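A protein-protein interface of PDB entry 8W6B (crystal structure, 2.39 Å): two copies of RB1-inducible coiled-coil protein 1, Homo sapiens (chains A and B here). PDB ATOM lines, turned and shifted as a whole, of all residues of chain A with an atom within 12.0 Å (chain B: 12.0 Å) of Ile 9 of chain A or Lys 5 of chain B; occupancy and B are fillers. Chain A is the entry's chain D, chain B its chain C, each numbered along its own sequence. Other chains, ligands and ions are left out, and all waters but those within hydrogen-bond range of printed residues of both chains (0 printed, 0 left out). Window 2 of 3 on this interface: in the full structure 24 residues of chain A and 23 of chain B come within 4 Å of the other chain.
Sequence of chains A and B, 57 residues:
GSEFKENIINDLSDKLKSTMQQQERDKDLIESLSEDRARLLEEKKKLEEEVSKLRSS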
ATOM      1  N   ASN A   7       0.824  31.493   0.261  1.00  0.00           N
ATOM      2  CA  ASN A   7       0.614  30.328   1.125  1.00  0.00           C
ATOM      3  C   ASN A   7       0.673  29.023   0.351  1.00  0.00           C
ATOM      4  O   ASN A   7       1.040  27.997   0.893  1.00  0.00           O
ATOM      5  CB  ASN A   7      -0.720  30.440   1.865  1.00  0.00           C
ATOM      6  CG  ASN A   7      -0.551  30.944   3.287  1.00  0.00           C
ATOM      7  OD1 ASN A   7       0.500  30.744   3.902  1.00  0.00           O
ATOM      8  ND2 ASN A   7      -1.575  31.611   3.811  1.00  0.00           N
ATOM      9  N   ILE A   8       0.319  29.049  -0.929  1.00  0.00           N
ATOM     10  CA  ILE A   8       0.535  27.856  -1.738  1.00  0.00           C
ATOM     11  C   ILE A   8       2.028  27.628  -1.950  1.00  0.00           C
ATOM     12  O   ILE A   8       2.511  26.496  -1.870  1.00  0.00           O
ATOM     13  CB  ILE A   8      -0.237  27.956  -3.065  1.00  0.00           C
ATOM     14  CG1 ILE A   8      -1.749  27.955  -2.797  1.00  0.00           C
ATOM     15  CG2 ILE A   8       0.134  26.796  -3.971  1.00  0.00           C
ATOM     16  CD1 ILE A   8      -2.410  29.332  -2.815  1.00  0.00           C
ATOM     17  N   ILE A   9       2.786  28.699  -2.186  1.00  0.00           N
ATOM     18  CA  ILE A   9       4.234  28.583  -2.375  1.00  0.00           C
ATOM     19  C   ILE A   9       4.919  28.153  -1.084  1.00  0.00           C
ATOM     20  O   ILE A   9       5.870  27.358  -1.104  1.00  0.00           O
ATOM     21  CB  ILE A   9       4.813  29.912  -2.905  1.00  0.00           C
ATOM     22  CG1 ILE A   9       4.600  30.020  -4.420  1.00  0.00           C
ATOM     23  CG2 ILE A   9       6.303  30.060  -2.541  1.00  0.00           C
ATOM     24  CD1 ILE A   9       4.561  31.437  -4.931  1.00  0.00           C
ATOM     25  N   ASN A  10       4.454  28.672   0.059  1.00  0.00           N
ATOM     26  CA  ASN A  10       5.027  28.284   1.347  1.00  0.00           C
ATOM     27  C   ASN A  10       4.874  26.793   1.589  1.00  0.00           C
ATOM     28  O   ASN A  10       5.845  26.100   1.915  1.00  0.00           O
ATOM     29  CB  ASN A  10       4.372  29.073   2.470  1.00  0.00           C
ATOM     30  CG  ASN A  10       4.632  30.541   2.359  1.00  0.00           C
ATOM     31  OD1 ASN A  10       5.490  31.073   3.056  1.00  0.00           O
ATOM     32  ND2 ASN A  10       3.893  31.215   1.482  1.00  0.00           N
ATOM     33  N   ASP A  11       3.658  26.276   1.421  1.00  0.00           N
ATOM     34  CA  ASP A  11       3.422  24.855   1.656  1.00  0.00           C
ATOM     35  C   ASP A  11       4.202  23.995   0.670  1.00  0.00           C
ATOM     36  O   ASP A  11       4.826  23.000   1.056  1.00  0.00           O
ATOM     37  CB  ASP A  11       1.923  24.567   1.580  1.00  0.00           C
ATOM     38  CG  ASP A  11       1.157  25.151   2.760  1.00  0.00           C
ATOM     39  OD1 ASP A  11       1.691  25.142   3.892  1.00  0.00           O
ATOM     40  OD2 ASP A  11       0.023  25.629   2.552  1.00  0.00           O
ATOM     41  N   LEU A  12       4.191  24.366  -0.608  1.00  0.00           N
ATOM     42  CA  LEU A  12       4.985  23.637  -1.589  1.00  0.00           C
ATOM     43  C   LEU A  12       6.452  23.624  -1.192  1.00  0.00           C
ATOM     44  O   LEU A  12       7.084  22.560  -1.141  1.00  0.00           O
ATOM     45  CB  LEU A  12       4.809  24.262  -2.978  1.00  0.00           C
ATOM     46  CG  LEU A  12       3.664  23.723  -3.845  1.00  0.00           C
ATOM     47  CD1 LEU A  12       2.316  23.778  -3.106  1.00  0.00           C
ATOM     48  CD2 LEU A  12       3.589  24.480  -5.173  1.00  0.00           C
ATOM     49  N   SER A  13       7.008  24.800  -0.879  1.00  0.00           N
ATOM     50  CA  SER A  13       8.439  24.865  -0.618  1.00  0.00           C
ATOM     51  C   SER A  13       8.813  24.141   0.679  1.00  0.00           C
ATOM     52  O   SER A  13       9.956  23.703   0.829  1.00  0.00           O
ATOM     53  CB  SER A  13       8.888  26.320  -0.593  1.00  0.00           C
ATOM     54  OG  SER A  13       9.965  26.496   0.291  1.00  0.00           O
ATOM     55  N   ASP A  14       7.870  23.988   1.623  1.00  0.00           N
ATOM     56  CA  ASP A  14       8.130  23.213   2.840  1.00  0.00           C
ATOM     57  C   ASP A  14       8.059  21.723   2.563  1.00  0.00           C
ATOM     58  O   ASP A  14       8.913  20.955   3.026  1.00  0.00           O
ATOM     59  CB  ASP A  14       7.136  23.580   3.946  1.00  0.00           C
ATOM     60  CG  ASP A  14       7.460  24.918   4.621  1.00  0.00           C
ATOM     61  OD1 ASP A  14       8.643  25.327   4.651  1.00  0.00           O
ATOM     62  OD2 ASP A  14       6.516  25.555   5.136  1.00  0.00           O
ATOM     63  N   LYS A  15       7.024  21.280   1.843  1.00  0.00           N
ATOM     64  CA  LYS A  15       6.931  19.854   1.545  1.00  0.00           C
ATOM     65  C   LYS A  15       8.084  19.421   0.653  1.00  0.00           C
ATOM     66  O   LYS A  15       8.699  18.376   0.888  1.00  0.00           O
ATOM     67  CB  LYS A  15       5.580  19.521   0.913  1.00  0.00           C
ATOM     68  CG  LYS A  15       4.388  19.788   1.828  1.00  0.00           C
ATOM     69  CD  LYS A  15       3.055  19.459   1.162  1.00  0.00           C
ATOM     70  CE  LYS A  15       2.289  20.731   0.819  1.00  0.00           C
ATOM     71  NZ  LYS A  15       0.811  20.531   0.771  1.00  0.00           N
ATOM     72  N   LEU A  16       8.424  20.231  -0.354  1.00  0.00           N
ATOM     73  CA  LEU A  16       9.629  19.953  -1.126  1.00  0.00           C
ATOM     74  C   LEU A  16      10.838  19.851  -0.210  1.00  0.00           C
ATOM     75  O   LEU A  16      11.641  18.922  -0.332  1.00  0.00           O
ATOM     76  CB  LEU A  16       9.848  21.027  -2.186  1.00  0.00           C
ATOM     77  CG  LEU A  16      10.972  20.693  -3.163  1.00  0.00           C
ATOM     78  CD1 LEU A  16      10.728  19.294  -3.741  1.00  0.00           C
ATOM     79  CD2 LEU A  16      11.074  21.754  -4.290  1.00  0.00           C
ATOM     80  N   LYS A  17      10.944  20.764   0.753  1.00  0.00           N
ATOM     81  CA  LYS A  17      12.064  20.753   1.687  1.00  0.00           C
ATOM     82  C   LYS A  17      12.121  19.441   2.458  1.00  0.00           C
ATOM     83  O   LYS A  17      13.144  18.747   2.461  1.00  0.00           O
ATOM     84  CB  LYS A  17      11.943  21.944   2.642  1.00  0.00           C
ATOM     85  CG  LYS A  17      13.143  22.176   3.517  1.00  0.00           C
ATOM     86  CD  LYS A  17      13.278  23.664   3.887  1.00  0.00           C
ATOM     87  CE  LYS A  17      12.176  24.132   4.841  1.00  0.00           C
ATOM     88  NZ  LYS A  17      12.037  25.641   4.882  1.00  0.00           N
ATOM     89  N   SER A  18      11.017  19.072   3.113  1.00  0.00           N
ATOM     90  CA  SER A  18      11.070  17.889   3.961  1.00  0.00           C
ATOM     91  C   SER A  18      11.204  16.627   3.120  1.00  0.00           C
ATOM     92  O   SER A  18      11.956  15.713   3.482  1.00  0.00           O
ATOM     93  CB  SER A  18       9.847  17.832   4.870  1.00  0.00           C
ATOM     94  OG  SER A  18       8.684  17.565   4.138  1.00  0.00           O
ATOM     95  N   THR A  19      10.523  16.582   1.973  1.00  0.00           N
ATOM     96  CA  THR A  19      10.645  15.437   1.075  1.00  0.00           C
ATOM     97  C   THR A  19      12.091  15.171   0.681  1.00  0.00           C
ATOM     98  O   THR A  19      12.528  14.015   0.653  1.00  0.00           O
ATOM     99  CB  THR A  19       9.804  15.647  -0.181  1.00  0.00           C
ATOM    100  OG1 THR A  19       8.430  15.851   0.186  1.00  0.00           O
ATOM    101  CG2 THR A  19       9.901  14.439  -1.066  1.00  0.00           C
ATOM    102  N   GLY B   1      -2.760  37.100  -8.209  1.00  0.00           N
ATOM    103  CA  GLY B   1      -1.685  36.276  -8.742  1.00  0.00           C
ATOM    104  C   GLY B   1      -1.281  36.675 -10.154  1.00  0.00           C
ATOM    105  O   GLY B   1      -2.014  37.407 -10.830  1.00  0.00           O
ATOM    106  N   SER B   2      -0.117  36.196 -10.601  1.00  0.00           N
ATOM    107  CA  SER B   2       0.461  36.566 -11.892  1.00  0.00           C
ATOM    108  C   SER B   2       0.970  35.313 -12.609  1.00  0.00           C
ATOM    109  O   SER B   2       0.962  34.204 -12.059  1.00  0.00           O
ATOM    110  CB  SER B   2       1.593  37.593 -11.718  1.00  0.00           C
ATOM    111  OG  SER B   2       2.566  37.157 -10.770  1.00  0.00           O
ATOM    112  N   GLU B   3       1.426  35.497 -13.855  1.00  0.00           N
ATOM    113  CA  GLU B   3       2.020  34.388 -14.599  1.00  0.00           C
ATOM    114  C   GLU B   3       3.403  34.027 -14.064  1.00  0.00           C
ATOM    115  O   GLU B   3       3.748  32.840 -13.989  1.00  0.00           O
ATOM    116  CB  GLU B   3       2.096  34.724 -16.090  1.00  0.00           C
ATOM    117  CG  GLU B   3       2.858  33.700 -16.947  1.00  0.00           C
ATOM    118  CD  GLU B   3       3.366  34.297 -18.263  1.00  0.00           C
ATOM    119  OE1 GLU B   3       4.353  35.064 -18.241  1.00  0.00           O
ATOM    120  OE2 GLU B   3       2.772  34.010 -19.325  1.00  0.00           O
ATOM    121  N   PHE B   4       4.207  35.034 -13.694  1.00  0.00           N
ATOM    122  CA  PHE B   4       5.502  34.770 -13.064  1.00  0.00           C
ATOM    123  C   PHE B   4       5.356  33.832 -11.879  1.00  0.00           C
ATOM    124  O   PHE B   4       6.160  32.905 -11.700  1.00  0.00           O
ATOM    125  CB  PHE B   4       6.154  36.084 -12.610  1.00  0.00           C
ATOM    126  CG  PHE B   4       7.493  35.897 -11.926  1.00  0.00           C
ATOM    127  CD1 PHE B   4       8.671  36.031 -12.642  1.00  0.00           C
ATOM    128  CD2 PHE B   4       7.571  35.600 -10.570  1.00  0.00           C
ATOM    129  CE1 PHE B   4       9.896  35.858 -12.030  1.00  0.00           C
ATOM    130  CE2 PHE B   4       8.800  35.420  -9.954  1.00  0.00           C
ATOM    131  CZ  PHE B   4       9.962  35.552 -10.692  1.00  0.00           C
ATOM    132  N   LYS B   5       4.342  34.078 -11.047  1.00  0.00           N
ATOM    133  CA  LYS B   5       4.136  33.272  -9.855  1.00  0.00           C
ATOM    134  C   LYS B   5       3.716  31.857 -10.220  1.00  0.00           C
ATOM    135  O   LYS B   5       4.208  30.891  -9.631  1.00  0.00           O
ATOM    136  CB  LYS B   5       3.089  33.938  -8.959  1.00  0.00           C
ATOM    137  CG  LYS B   5       2.703  33.146  -7.718  1.00  0.00           C
ATOM    138  CD  LYS B   5       1.630  33.886  -6.933  1.00  0.00           C
ATOM    139  CE  LYS B   5       0.602  32.939  -6.331  1.00  0.00           C
ATOM    140  NZ  LYS B   5      -0.205  33.611  -5.269  1.00  0.00           N
ATOM    141  N   GLU B   6       2.819  31.712 -11.201  1.00  0.00           N
ATOM    142  CA  GLU B   6       2.265  30.397 -11.513  1.00  0.00           C
ATOM    143  C   GLU B   6       3.307  29.468 -12.120  1.00  0.00           C
ATOM    144  O   GLU B   6       3.242  28.252 -11.897  1.00  0.00           O
ATOM    145  CB  GLU B   6       1.056  30.530 -12.446  1.00  0.00           C
ATOM    146  CG  GLU B   6      -0.176  31.181 -11.815  1.00  0.00           C
ATOM    147  CD  GLU B   6      -0.886  30.268 -10.819  1.00  0.00           C
ATOM    148  OE1 GLU B   6      -1.028  29.059 -11.104  1.00  0.00           O
ATOM    149  OE2 GLU B   6      -1.292  30.760  -9.742  1.00  0.00           O
ATOM    150  N   ASN B   7       4.275  30.015 -12.872  1.00  0.00           N
ATOM    151  CA  ASN B   7       5.320  29.184 -13.471  1.00  0.00           C
ATOM    152  C   ASN B   7       6.211  28.561 -12.412  1.00  0.00           C
ATOM    153  O   ASN B   7       6.753  27.469 -12.617  1.00  0.00           O
ATOM    154  CB  ASN B   7       6.171  29.997 -14.446  1.00  0.00           C
ATOM    155  CG  ASN B   7       5.394  30.430 -15.676  1.00  0.00           C
ATOM    156  OD1 ASN B   7       4.288  29.946 -15.926  1.00  0.00           O
ATOM    157  ND2 ASN B   7       5.973  31.344 -16.456  1.00  0.00           N
ATOM    158  N   ILE B   8       6.376  29.233 -11.279  1.00  0.00           N
ATOM    159  CA  ILE B   8       7.168  28.678 -10.192  1.00  0.00           C
ATOM    160  C   ILE B   8       6.341  27.730  -9.328  1.00  0.00           C
ATOM    161  O   ILE B   8       6.845  26.692  -8.887  1.00  0.00           O
ATOM    162  CB  ILE B   8       7.783  29.826  -9.376  1.00  0.00           C
ATOM    163  CG1 ILE B   8       8.804  30.546 -10.251  1.00  0.00           C
ATOM    164  CG2 ILE B   8       8.444  29.287  -8.132  1.00  0.00           C
ATOM    165  CD1 ILE B   8       9.563  31.613  -9.559  1.00  0.00           C
ATOM    166  N   ILE B   9       5.072  28.072  -9.076  1.00  0.00           N
ATOM    167  CA  ILE B   9       4.135  27.109  -8.497  1.00  0.00           C
ATOM    168  C   ILE B   9       4.199  25.800  -9.276  1.00  0.00           C
ATOM    169  O   ILE B   9       4.516  24.741  -8.722  1.00  0.00           O
ATOM    170  CB  ILE B   9       2.706  27.685  -8.485  1.00  0.00           C
ATOM    171  CG1 ILE B   9       2.535  28.710  -7.359  1.00  0.00           C
ATOM    172  CG2 ILE B   9       1.657  26.568  -8.373  1.00  0.00           C
ATOM    173  CD1 ILE B   9       1.159  29.383  -7.345  1.00  0.00           C
ATOM    174  N   ASN B  10       3.949  25.875 -10.592  1.00  0.00           N
ATOM    175  CA  ASN B  10       3.980  24.687 -11.449  1.00  0.00           C
ATOM    176  C   ASN B  10       5.331  23.990 -11.396  1.00  0.00           C
ATOM    177  O   ASN B  10       5.394  22.758 -11.303  1.00  0.00           O
ATOM    178  CB  ASN B  10       3.637  25.057 -12.896  1.00  0.00           C
ATOM    179  CG  ASN B  10       2.196  25.492 -13.053  1.00  0.00           C
ATOM    180  OD1 ASN B  10       1.393  25.293 -12.147  1.00  0.00           O
ATOM    181  ND2 ASN B  10       1.862  26.106 -14.190  1.00  0.00           N
ATOM    182  N   ASP B  11       6.424  24.758 -11.462  1.00  0.00           N
ATOM    183  CA  ASP B  11       7.748  24.154 -11.353  1.00  0.00           C
ATOM    184  C   ASP B  11       7.918  23.464 -10.004  1.00  0.00           C
ATOM    185  O   ASP B  11       8.386  22.321  -9.932  1.00  0.00           O
ATOM    186  CB  ASP B  11       8.835  25.209 -11.562  1.00  0.00           C
ATOM    187  CG  ASP B  11      10.219  24.596 -11.694  1.00  0.00           C
ATOM    188  OD1 ASP B  11      10.517  24.068 -12.788  1.00  0.00           O
ATOM    189  OD2 ASP B  11      11.007  24.646 -10.717  1.00  0.00           O
ATOM    190  N   LEU B  12       7.518  24.135  -8.921  1.00  0.00           N
ATOM    191  CA  LEU B  12       7.653  23.525  -7.603  1.00  0.00           C
ATOM    192  C   LEU B  12       6.760  22.290  -7.478  1.00  0.00           C
ATOM    193  O   LEU B  12       7.211  21.240  -6.993  1.00  0.00           O
ATOM    194  CB  LEU B  12       7.340  24.553  -6.513  1.00  0.00           C
ATOM    195  CG  LEU B  12       8.368  25.634  -6.137  1.00  0.00           C
ATOM    196  CD1 LEU B  12       8.006  26.273  -4.787  1.00  0.00           C
ATOM    197  CD2 LEU B  12       9.802  25.085  -6.121  1.00  0.00           C
ATOM    198  N   SER B  13       5.501  22.379  -7.942  1.00  0.00           N
ATOM    199  CA  SER B  13       4.595  21.233  -7.842  1.00  0.00           C
ATOM    200  C   SER B  13       5.070  20.055  -8.690  1.00  0.00           C
ATOM    201  O   SER B  13       4.906  18.901  -8.293  1.00  0.00           O
ATOM    202  CB  SER B  13       3.178  21.610  -8.260  1.00  0.00           C
ATOM    203  OG  SER B  13       2.870  22.934  -7.874  1.00  0.00           O
ATOM    204  N   ASP B  14       5.659  20.313  -9.855  1.00  0.00           N
ATOM    205  CA  ASP B  14       6.195  19.216 -10.655  1.00  0.00           C
ATOM    206  C   ASP B  14       7.294  18.476  -9.901  1.00  0.00           C
ATOM    207  O   ASP B  14       7.206  17.258  -9.706  1.00  0.00           O
ATOM    208  CB  ASP B  14       6.699  19.741 -12.001  1.00  0.00           C
ATOM    209  CG  ASP B  14       5.570  19.979 -12.982  1.00  0.00           C
ATOM    210  OD1 ASP B  14       5.830  20.547 -14.068  1.00  0.00           O
ATOM    211  OD2 ASP B  14       4.415  19.619 -12.655  1.00  0.00           O
ATOM    212  N   LYS B  15       8.329  19.203  -9.447  1.00  0.00           N
ATOM    213  CA  LYS B  15       9.427  18.554  -8.730  1.00  0.00           C
ATOM    214  C   LYS B  15       8.941  17.868  -7.459  1.00  0.00           C
ATOM    215  O   LYS B  15       9.419  16.783  -7.125  1.00  0.00           O
ATOM    216  CB  LYS B  15      10.538  19.549  -8.402  1.00  0.00           C
ATOM    217  CG  LYS B  15      10.957  20.374  -9.578  1.00  0.00           C
ATOM    218  CD  LYS B  15      11.614  21.669  -9.161  1.00  0.00           C
ATOM    219  CE  LYS B  15      12.841  21.949 -10.018  1.00  0.00           C
ATOM    220  NZ  LYS B  15      13.343  23.356  -9.850  1.00  0.00           N
ATOM    221  N   LEU B  16       7.998  18.477  -6.738  1.00  0.00           N
ATOM    222  CA  LEU B  16       7.445  17.823  -5.552  1.00  0.00           C
ATOM    223  C   LEU B  16       6.785  16.498  -5.915  1.00  0.00           C
ATOM    224  O   LEU B  16       6.996  15.481  -5.240  1.00  0.00           O
ATOM    225  CB  LEU B  16       6.446  18.742  -4.838  1.00  0.00           C
ATOM    226  CG  LEU B  16       5.611  18.130  -3.706  1.00  0.00           C
ATOM    227  CD1 LEU B  16       6.487  17.757  -2.523  1.00  0.00           C
ATOM    228  CD2 LEU B  16       4.519  19.095  -3.253  1.00  0.00           C
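Of the 16 printed residues of chain B, 5 touch a printed residue of chain A.
Of the 13 printed residues of chain A, 5 touch a printed residue of chain B.
Hydrophobic or aromatic side chains of chain A within 4 Å of the printed part of chain B: Ile 9 and Leu 12.
Among the printed residues, 8 pairs touch across the chains.
No residue of chain B comes within 4 Å of Ile 8 of chain A.
Of chain B, only Lys 5 and Ile 9 come within 4 Å of Ile 9 of chain A.
No residue of chain B comes within 4 Å of Asn 10 of chain A.
No residue of chain B comes within 4 Å of Asp 11 of chain A.
No residue of chain B comes within 4 Å of Ser 13 of chain A.
Of the printed residues of chain B, Thr 19 of chain A touches Leu 16 (3.8 Å).
No residue of chain A comes within 4 Å of Gly 1 of chain B.
Glu 3 of chain B touches none of the printed residues of chain A.
No residue of chain A comes within 4 Å of Phe 4 of chain B.
No residue of chain A comes within 4 Å of Glu 6 of chain B.
No residue of chain A comes within 4 Å of Ile 8 of chain B.
Ile 9 of chain B touches just these residues of chain A: Ile 9 (3.8 Å) and Leu 12 (3.7 Å).
Printed residues of chain A within 4 Å of Leu 12 of chain B: Leu 12.
Of the printed residues of chain A, Ser 13 of chain B touches Leu 12.
Of the printed residues of chain A, Leu 16 of chain B touches Lys 15, Leu 16 and Thr 19.
The nearest printed residue of chain B that does not touch Leu 12 of chain A is Leu 16 of chain B (4.7 Å).
Ile 9 of chain A touches Lys 5 of chain B (CD1 to CG, 3.8 Å).
Ile 9 of chain A touches Ile 9 of chain B (CG1 to CG1, 3.8 Å).
Leu 12 of chain A touches Ile 9 of chain B (CD2 to O, 3.7 Å).
Leu 12 of chain B touches Leu 12 of chain A.
OG of Ser 13 of chain B touches CD2 of Leu 12 of chain A, at 3.2 Å.
Leu 16 of chain B touches Lys 15 of chain A (CD1 to C, 3.9 Å).
Leu 16 of chain B touches Leu 16 of chain A.
Leu 16 of chain B touches Thr 19 of chain A.
Ile 9 of chain A touches its own counterpart, Ile 9 of chain B.
Leu 12 of chain A touches Ile 9 of chain B, but with the chains exchanged Ile 9 of chain A does not touch Leu 12 of chain B (4.4 Å).
Lys 15 of chain A touches Leu 16 of chain B, but with the chains exchanged Leu 16 of chain A does not touch Lys 15 of chain B (4.4 Å).
Leu 16 of chain B touches its own counterpart, Leu 16 of chain A.
Positions printed for both chains: 7, 8, 9, 10, 11, 12, 13, 14, 15 and 16.
Of the 8 pairs that touch across the chains among the printed residues, 3 have their exchanged pair printed and touching as well.
The backbone carbonyl oxygen of Lys 15 of chain A is in hydrogen-bond range of the side-chain hydroxyl of Thr 19 of chain A, 2.6 Å away.
The backbone carbonyl oxygen of Ile 9 of chain B is in hydrogen-bond range of the side-chain hydroxyl of Ser 13 of chain B, at 2.6 Å.
The side-chain hydroxyl (OG) of Ser 18 of chain A sits at hydrogen-bond distance from the backbone carbonyl oxygen (O) of Lys 15 of chain A, at 3.3 Å.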
